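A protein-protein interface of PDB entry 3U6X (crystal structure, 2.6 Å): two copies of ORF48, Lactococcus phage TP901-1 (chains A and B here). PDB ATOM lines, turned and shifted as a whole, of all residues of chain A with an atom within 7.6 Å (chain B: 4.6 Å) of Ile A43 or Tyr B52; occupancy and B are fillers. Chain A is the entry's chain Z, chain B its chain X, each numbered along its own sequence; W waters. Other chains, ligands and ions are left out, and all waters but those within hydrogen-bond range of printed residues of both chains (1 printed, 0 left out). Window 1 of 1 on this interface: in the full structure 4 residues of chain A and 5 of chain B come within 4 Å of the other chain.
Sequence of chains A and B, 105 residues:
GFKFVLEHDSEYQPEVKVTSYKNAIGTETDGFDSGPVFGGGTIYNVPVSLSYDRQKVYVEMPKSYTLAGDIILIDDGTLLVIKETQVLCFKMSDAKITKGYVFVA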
ATOM      1  N   VAL A  18      26.163  -1.541  29.886  1.00  0.00           N
ATOM      2  CA  VAL A  18      25.483  -0.245  29.917  1.00  0.00           C
ATOM      3  C   VAL A  18      24.773   0.056  28.590  1.00  0.00           C
ATOM      4  O   VAL A  18      25.284  -0.248  27.507  1.00  0.00           O
ATOM      5  CB  VAL A  18      26.388   0.910  30.429  1.00  0.00           C
ATOM      6  CG1 VAL A  18      25.575   2.160  30.738  1.00  0.00           C
ATOM      7  CG2 VAL A  18      27.168   0.493  31.670  1.00  0.00           C
ATOM      8  N   THR A  19      23.523   0.547  28.707  1.00  0.00           N
ATOM      9  CA  THR A  19      22.648   0.915  27.589  1.00  0.00           C
ATOM     10  C   THR A  19      21.986   2.285  27.827  1.00  0.00           C
ATOM     11  O   THR A  19      21.758   2.686  28.965  1.00  0.00           O
ATOM     12  CB  THR A  19      21.601  -0.169  27.263  1.00  0.00           C
ATOM     13  OG1 THR A  19      20.780  -0.386  28.404  1.00  0.00           O
ATOM     14  CG2 THR A  19      22.208  -1.479  26.762  1.00  0.00           C
ATOM     15  N   SER A  20      21.724   3.004  26.736  1.00  0.00           N
ATOM     16  CA  SER A  20      21.089   4.313  26.758  1.00  0.00           C
ATOM     17  C   SER A  20      19.887   4.257  25.828  1.00  0.00           C
ATOM     18  O   SER A  20      19.977   3.712  24.721  1.00  0.00           O
ATOM     19  CB  SER A  20      22.047   5.424  26.306  1.00  0.00           C
ATOM     20  OG  SER A  20      21.529   6.687  26.716  1.00  0.00           O
ATOM     21  N   TYR A  21      18.768   4.843  26.273  1.00  0.00           N
ATOM     22  CA  TYR A  21      17.516   4.876  25.514  1.00  0.00           C
ATOM     23  C   TYR A  21      16.588   5.984  26.024  1.00  0.00           C
ATOM     24  O   TYR A  21      16.689   6.415  27.182  1.00  0.00           O
ATOM     25  CB  TYR A  21      16.802   3.485  25.510  1.00  0.00           C
ATOM     26  CG  TYR A  21      16.703   2.824  26.875  1.00  0.00           C
ATOM     27  CD1 TYR A  21      17.697   1.959  27.329  1.00  0.00           C
ATOM     28  CD2 TYR A  21      15.620   3.073  27.717  1.00  0.00           C
ATOM     29  CE1 TYR A  21      17.643   1.401  28.609  1.00  0.00           C
ATOM     30  CE2 TYR A  21      15.532   2.484  28.978  1.00  0.00           C
ATOM     31  CZ  TYR A  21      16.549   1.656  29.425  1.00  0.00           C
ATOM     32  OH  TYR A  21      16.455   1.089  30.674  1.00  0.00           O
ATOM     33  N   LYS A  22      15.679   6.430  25.130  1.00  0.00           N
ATOM     34  CA  LYS A  22      14.679   7.486  25.321  1.00  0.00           C
ATOM     35  C   LYS A  22      13.242   6.873  25.263  1.00  0.00           C
ATOM     36  O   LYS A  22      13.009   5.885  24.554  1.00  0.00           O
ATOM     37  CB  LYS A  22      14.888   8.515  24.202  1.00  0.00           C
ATOM     38  CG  LYS A  22      14.206   9.863  24.347  1.00  0.00           C
ATOM     39  CD  LYS A  22      14.615  10.755  23.177  1.00  0.00           C
ATOM     40  CE  LYS A  22      13.528  11.701  22.718  1.00  0.00           C
ATOM     41  NZ  LYS A  22      13.691  12.075  21.279  1.00  0.00           N
ATOM     42  N   GLY A  39       7.447   0.957  23.586  1.00  0.00           N
ATOM     43  CA  GLY A  39       8.418   0.387  24.533  1.00  0.00           C
ATOM     44  C   GLY A  39       9.636   1.249  24.860  1.00  0.00           C
ATOM     45  O   GLY A  39      10.253   1.069  25.910  1.00  0.00           O
ATOM     46  N   GLY A  40       9.957   2.179  23.956  1.00  0.00           N
ATOM     47  CA  GLY A  40      11.061   3.124  23.999  1.00  0.00           C
ATOM     48  C   GLY A  40      11.709   3.211  22.632  1.00  0.00           C
ATOM     49  O   GLY A  40      11.461   2.362  21.767  1.00  0.00           O
ATOM     50  N   GLY A  41      12.569   4.205  22.450  1.00  0.00           N
ATOM     51  CA  GLY A  41      13.279   4.392  21.195  1.00  0.00           C
ATOM     52  C   GLY A  41      14.419   3.409  20.987  1.00  0.00           C
ATOM     53  O   GLY A  41      14.422   2.311  21.565  1.00  0.00           O
ATOM     54  N   THR A  42      15.409   3.808  20.159  1.00  0.00           N
ATOM     55  CA  THR A  42      16.591   3.011  19.830  1.00  0.00           C
ATOM     56  C   THR A  42      17.401   2.774  21.089  1.00  0.00           C
ATOM     57  O   THR A  42      17.603   3.716  21.856  1.00  0.00           O
ATOM     58  CB  THR A  42      17.404   3.679  18.694  1.00  0.00           C
ATOM     59  OG1 THR A  42      16.540   3.897  17.575  1.00  0.00           O
ATOM     60  CG2 THR A  42      18.590   2.834  18.242  1.00  0.00           C
ATOM     61  N   ILE A  43      17.818   1.507  21.322  1.00  0.00           N
ATOM     62  CA  ILE A  43      18.653   1.124  22.467  1.00  0.00           C
ATOM     63  C   ILE A  43      20.106   1.172  22.013  1.00  0.00           C
ATOM     64  O   ILE A  43      20.494   0.456  21.088  1.00  0.00           O
ATOM     65  CB  ILE A  43      18.271  -0.270  23.041  1.00  0.00           C
ATOM     66  CG1 ILE A  43      16.874  -0.224  23.669  1.00  0.00           C
ATOM     67  CG2 ILE A  43      19.335  -0.747  24.069  1.00  0.00           C
ATOM     68  CD1 ILE A  43      16.193  -1.524  23.748  1.00  0.00           C
ATOM     69  N   TYR A  44      20.886   2.034  22.628  1.00  0.00           N
ATOM     70  CA  TYR A  44      22.304   2.155  22.286  1.00  0.00           C
ATOM     71  C   TYR A  44      23.177   1.465  23.304  1.00  0.00           C
ATOM     72  O   TYR A  44      23.009   1.719  24.504  1.00  0.00           O
ATOM     73  CB  TYR A  44      22.723   3.626  22.124  1.00  0.00           C
ATOM     74  CG  TYR A  44      21.947   4.348  21.046  1.00  0.00           C
ATOM     75  CD1 TYR A  44      22.415   4.394  19.734  1.00  0.00           C
ATOM     76  CD2 TYR A  44      20.768   5.034  21.345  1.00  0.00           C
ATOM     77  CE1 TYR A  44      21.715   5.076  18.737  1.00  0.00           C
ATOM     78  CE2 TYR A  44      20.064   5.727  20.360  1.00  0.00           C
ATOM     79  CZ  TYR A  44      20.530   5.728  19.050  1.00  0.00           C
ATOM     80  OH  TYR A  44      19.833   6.390  18.062  1.00  0.00           O
ATOM     81  N   ASN A  45      24.091   0.574  22.828  1.00  0.00           N
ATOM     82  CA  ASN A  45      25.069  -0.092  23.687  1.00  0.00           C
ATOM     83  C   ASN A  45      26.176   0.909  23.959  1.00  0.00           C
ATOM     84  O   ASN A  45      26.832   1.372  23.023  1.00  0.00           O
ATOM     85  CB  ASN A  45      25.645  -1.337  23.028  1.00  0.00           C
ATOM     86  CG  ASN A  45      24.716  -2.528  22.969  1.00  0.00           C
ATOM     87  OD1 ASN A  45      23.593  -2.513  23.496  1.00  0.00           O
ATOM     88  ND2 ASN A  45      25.175  -3.595  22.317  1.00  0.00           N
ATOM     89  N   VAL A  46      26.327   1.308  25.227  1.00  0.00           N
ATOM     90  CA  VAL A  46      27.354   2.240  25.682  1.00  0.00           C
ATOM     91  C   VAL A  46      28.694   1.492  25.839  1.00  0.00           C
ATOM     92  O   VAL A  46      28.729   0.489  26.548  1.00  0.00           O
ATOM     93  CB  VAL A  46      26.930   2.898  27.016  1.00  0.00           C
ATOM     94  CG1 VAL A  46      27.957   3.947  27.473  1.00  0.00           C
ATOM     95  CG2 VAL A  46      25.529   3.495  26.898  1.00  0.00           C
ATOM     96  N   CYS A  89      21.119   2.825  31.607  1.00  0.00           N
ATOM     97  CA  CYS A  89      20.821   1.542  32.267  1.00  0.00           C
ATOM     98  C   CYS A  89      22.041   0.657  32.532  1.00  0.00           C
ATOM     99  O   CYS A  89      22.723   0.257  31.583  1.00  0.00           O
ATOM    100  CB  CYS A  89      19.763   0.794  31.458  1.00  0.00           C
ATOM    101  SG  CYS A  89      19.338  -0.835  32.112  1.00  0.00           S
ATOM    102  N   GLN B  13      17.197  -7.826  22.150  1.00  0.00           N
ATOM    103  CA  GLN B  13      18.417  -7.249  21.599  1.00  0.00           C
ATOM    104  C   GLN B  13      19.489  -8.321  21.464  1.00  0.00           C
ATOM    105  O   GLN B  13      20.393  -8.386  22.303  1.00  0.00           O
ATOM    106  CB  GLN B  13      18.909  -6.040  22.438  1.00  0.00           C
ATOM    107  CG  GLN B  13      17.944  -4.860  22.489  1.00  0.00           C
ATOM    108  CD  GLN B  13      16.843  -5.077  23.473  1.00  0.00           C
ATOM    109  OE1 GLN B  13      17.065  -5.524  24.601  1.00  0.00           O
ATOM    110  NE2 GLN B  13      15.630  -4.814  23.042  1.00  0.00           N
ATOM    111  N   PRO B  14      19.411  -9.176  20.418  1.00  0.00           N
ATOM    112  CA  PRO B  14      20.401 -10.252  20.271  1.00  0.00           C
ATOM    113  C   PRO B  14      21.826  -9.788  20.050  1.00  0.00           C
ATOM    114  O   PRO B  14      22.045  -8.819  19.336  1.00  0.00           O
ATOM    115  CB  PRO B  14      19.878 -11.051  19.078  1.00  0.00           C
ATOM    116  CG  PRO B  14      19.035 -10.140  18.351  1.00  0.00           C
ATOM    117  CD  PRO B  14      18.394  -9.262  19.357  1.00  0.00           C
ATOM    118  N   GLU B  15      22.788 -10.451  20.707  1.00  0.00           N
ATOM    119  CA  GLU B  15      24.206 -10.147  20.563  1.00  0.00           C
ATOM    120  C   GLU B  15      24.657 -10.550  19.156  1.00  0.00           C
ATOM    121  O   GLU B  15      24.241 -11.590  18.634  1.00  0.00           O
ATOM    122  CB  GLU B  15      25.029 -10.902  21.605  1.00  0.00           C
ATOM    123  CG  GLU B  15      25.832 -10.011  22.535  1.00  0.00           C
ATOM    124  CD  GLU B  15      26.802  -9.042  21.879  1.00  0.00           C
ATOM    125  OE1 GLU B  15      26.451  -7.842  21.790  1.00  0.00           O
ATOM    126  OE2 GLU B  15      27.914  -9.469  21.482  1.00  0.00           O
ATOM    127  N   VAL B  16      25.462  -9.687  18.531  1.00  0.00           N
ATOM    128  CA  VAL B  16      25.986  -9.917  17.189  1.00  0.00           C
ATOM    129  C   VAL B  16      27.506  -9.860  17.289  1.00  0.00           C
ATOM    130  O   VAL B  16      28.069  -8.964  17.931  1.00  0.00           O
ATOM    131  CB  VAL B  16      25.422  -8.905  16.139  1.00  0.00           C
ATOM    132  CG1 VAL B  16      26.018  -9.138  14.751  1.00  0.00           C
ATOM    133  CG2 VAL B  16      23.903  -8.973  16.067  1.00  0.00           C
ATOM    134  N   LEU B  50      26.927  -1.736  18.553  1.00  0.00           N
ATOM    135  CA  LEU B  50      25.554  -2.197  18.365  1.00  0.00           C
ATOM    136  C   LEU B  50      24.477  -1.225  18.897  1.00  0.00           C
ATOM    137  O   LEU B  50      24.630  -0.545  19.928  1.00  0.00           O
ATOM    138  CB  LEU B  50      25.350  -3.650  18.857  1.00  0.00           C
ATOM    139  CG  LEU B  50      26.352  -4.689  18.339  1.00  0.00           C
ATOM    140  CD1 LEU B  50      26.160  -6.000  19.011  1.00  0.00           C
ATOM    141  CD2 LEU B  50      26.279  -4.843  16.849  1.00  0.00           C
ATOM    142  N   SER B  51      23.398  -1.162  18.132  1.00  0.00           N
ATOM    143  CA  SER B  51      22.260  -0.277  18.295  1.00  0.00           C
ATOM    144  C   SER B  51      21.002  -1.102  17.928  1.00  0.00           C
ATOM    145  O   SER B  51      21.029  -1.844  16.938  1.00  0.00           O
ATOM    146  CB  SER B  51      22.426   0.874  17.307  1.00  0.00           C
ATOM    147  OG  SER B  51      21.834   2.056  17.796  1.00  0.00           O
ATOM    148  N   TYR B  52      19.897  -0.941  18.684  1.00  0.00           N
ATOM    149  CA  TYR B  52      18.699  -1.753  18.449  1.00  0.00           C
ATOM    150  C   TYR B  52      17.349  -1.062  18.359  1.00  0.00           C
ATOM    151  O   TYR B  52      16.968  -0.260  19.225  1.00  0.00           O
ATOM    152  CB  TYR B  52      18.574  -2.824  19.561  1.00  0.00           C
ATOM    153  CG  TYR B  52      19.740  -3.771  19.695  1.00  0.00           C
ATOM    154  CD1 TYR B  52      19.751  -4.985  19.023  1.00  0.00           C
ATOM    155  CD2 TYR B  52      20.819  -3.469  20.526  1.00  0.00           C
ATOM    156  CE1 TYR B  52      20.807  -5.879  19.165  1.00  0.00           C
ATOM    157  CE2 TYR B  52      21.899  -4.335  20.642  1.00  0.00           C
ATOM    158  CZ  TYR B  52      21.876  -5.550  19.977  1.00  0.00           C
ATOM    159  OH  TYR B  52      22.898  -6.446  20.093  1.00  0.00           O
ATOM    160  N   ASP B  53      16.572  -1.509  17.377  1.00  0.00           N
ATOM    161  CA  ASP B  53      15.156  -1.193  17.174  1.00  0.00           C
ATOM    162  C   ASP B  53      14.411  -2.538  17.194  1.00  0.00           C
ATOM    163  O   ASP B  53      15.076  -3.589  17.244  1.00  0.00           O
ATOM    164  CB  ASP B  53      14.929  -0.464  15.842  1.00  0.00           C
ATOM    165  CG  ASP B  53      15.117   1.044  15.898  1.00  0.00           C
ATOM    166  OD1 ASP B  53      15.037   1.624  17.020  1.00  0.00           O
ATOM    167  OD2 ASP B  53      15.322   1.653  14.822  1.00  0.00           O
ATOM    168  N   LYS B  56      15.517  -5.269  14.560  1.00  0.00           N
ATOM    169  CA  LYS B  56      16.552  -4.630  13.744  1.00  0.00           C
ATOM    170  C   LYS B  56      17.773  -4.332  14.600  1.00  0.00           C
ATOM    171  O   LYS B  56      17.648  -3.688  15.644  1.00  0.00           O
ATOM    172  CB  LYS B  56      16.014  -3.308  13.158  1.00  0.00           C
ATOM    173  CG  LYS B  56      15.831  -3.303  11.645  1.00  0.00           C
ATOM    174  CD  LYS B  56      15.021  -2.081  11.149  1.00  0.00           C
ATOM    175  CE  LYS B  56      13.524  -2.329  11.133  1.00  0.00           C
ATOM    176  NZ  LYS B  56      13.102  -3.133   9.950  1.00  0.00           N
ATOM    177  N   VAL B  57      18.952  -4.803  14.156  1.00  0.00           N
ATOM    178  CA  VAL B  57      20.229  -4.527  14.803  1.00  0.00           C
ATOM    179  C   VAL B  57      21.003  -3.635  13.836  1.00  0.00           C
ATOM    180  O   VAL B  57      21.163  -3.985  12.666  1.00  0.00           O
ATOM    181  CB  VAL B  57      21.065  -5.804  15.128  1.00  0.00           C
ATOM    182  CG1 VAL B  57      22.242  -5.464  16.028  1.00  0.00           C
ATOM    183  CG2 VAL B  57      20.218  -6.871  15.777  1.00  0.00           C
ATOM    184  N   TYR B  58      21.508  -2.511  14.332  1.00  0.00           N
ATOM    185  CA  TYR B  58      22.379  -1.642  13.555  1.00  0.00           C
ATOM    186  C   TYR B  58      23.814  -1.947  13.990  1.00  0.00           C
ATOM    187  O   TYR B  58      24.141  -1.773  15.158  1.00  0.00           O
ATOM    188  CB  TYR B  58      22.003  -0.175  13.749  1.00  0.00           C
ATOM    189  CG  TYR B  58      20.545   0.097  13.457  1.00  0.00           C
ATOM    190  CD1 TYR B  58      20.088   0.231  12.147  1.00  0.00           C
ATOM    191  CD2 TYR B  58      19.623   0.246  14.490  1.00  0.00           C
ATOM    192  CE1 TYR B  58      18.738   0.459  11.873  1.00  0.00           C
ATOM    193  CE2 TYR B  58      18.276   0.489  14.229  1.00  0.00           C
ATOM    194  CZ  TYR B  58      17.838   0.595  12.920  1.00  0.00           C
ATOM    195  OH  TYR B  58      16.509   0.831  12.676  1.00  0.00           O
HETATM  196  O   HOH W   1      14.569  -0.526  20.502  1.00  0.00           O
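The backbone NH of Tyr B52 is in hydrogen-bond range of the backbone carbonyl oxygen of Ile A43. O of Leu B50 sits at hydrogen-bond distance from N of Asn A45. The side-chain carboxylate (OD1) of Asp B53 lies within hydrogen-bond range of the side-chain hydroxyl (OG1) of Thr A42 (2.8 Å).
The backbone NH (N) of Tyr B58 lies within hydrogen-bond range of the backbone carbonyl oxygen (O) of Ser B51, 2.7 Å away. O of Ser A20 sits at hydrogen-bond distance from N of Tyr A44, at 2.8 Å. The side-chain hydroxyl of Tyr B58 is in hydrogen-bond range of the side-chain carboxylate of Asp B53 (2.6 Å). OH of Tyr B52 is in hydrogen-bond range of O of Pro B14, 2.6 Å away.
Printed residues of chain A that touch a printed residue of chain B: Thr A42, Ile A43, Tyr A44 and Asn A45. Hydrophobic or aromatic side chains of chain A that line the printed part of chain B: Ile A43 and Tyr A44. Among the printed residues, no Asp or Glu carboxylate lies within 4 Å of a Lys or Arg side-chain nitrogen of the other chain.
No position is printed for both chains. Of the 9 pairs that touch across the chains among the printed residues, none has its exchanged pair printed and touching as well.
Of chain B, only Gln B13, Ser B51 and Tyr B52 come within 4 Å of Ile A43. Of the printed residues of chain B, Asn A45 touches Leu B50 and Tyr B52. Of the printed residues of chain A, Leu B50 touches Asn A45 (3.2 Å). Of chain A, only Thr A42, Ile A43 and Asn A45 come within 4 Å of Tyr B52. Lys B56 touches none of the printed residues of chain A. Tyr B58 touches none of the printed residues of chain A. The nearest residue of chain B that does not touch Ile A43 is Leu B50 (4.4 Å). The nearest printed residue of chain A that does not touch Asp B53 is Gly A41 (4.4 Å).
Thr A42 touches Ser B51 (CG2 to OG, 3.4 Å). Tyr B52 touches Thr A42 (O to CA, 3.3 Å). Ile A43 touches Gln B13 (CD1 to NE2, 3.4 Å). CA of Ser B51 touches O of Ile A43, 3.4 Å away. CD1 of Tyr A44 touches OG of Ser B51, at 3.1 Å. CE2 of Tyr B52 touches ND2 of Asn A45, at 3.8 Å.
Water W1 lies within hydrogen-bond range of O of Tyr B52 and O of Gly A41.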
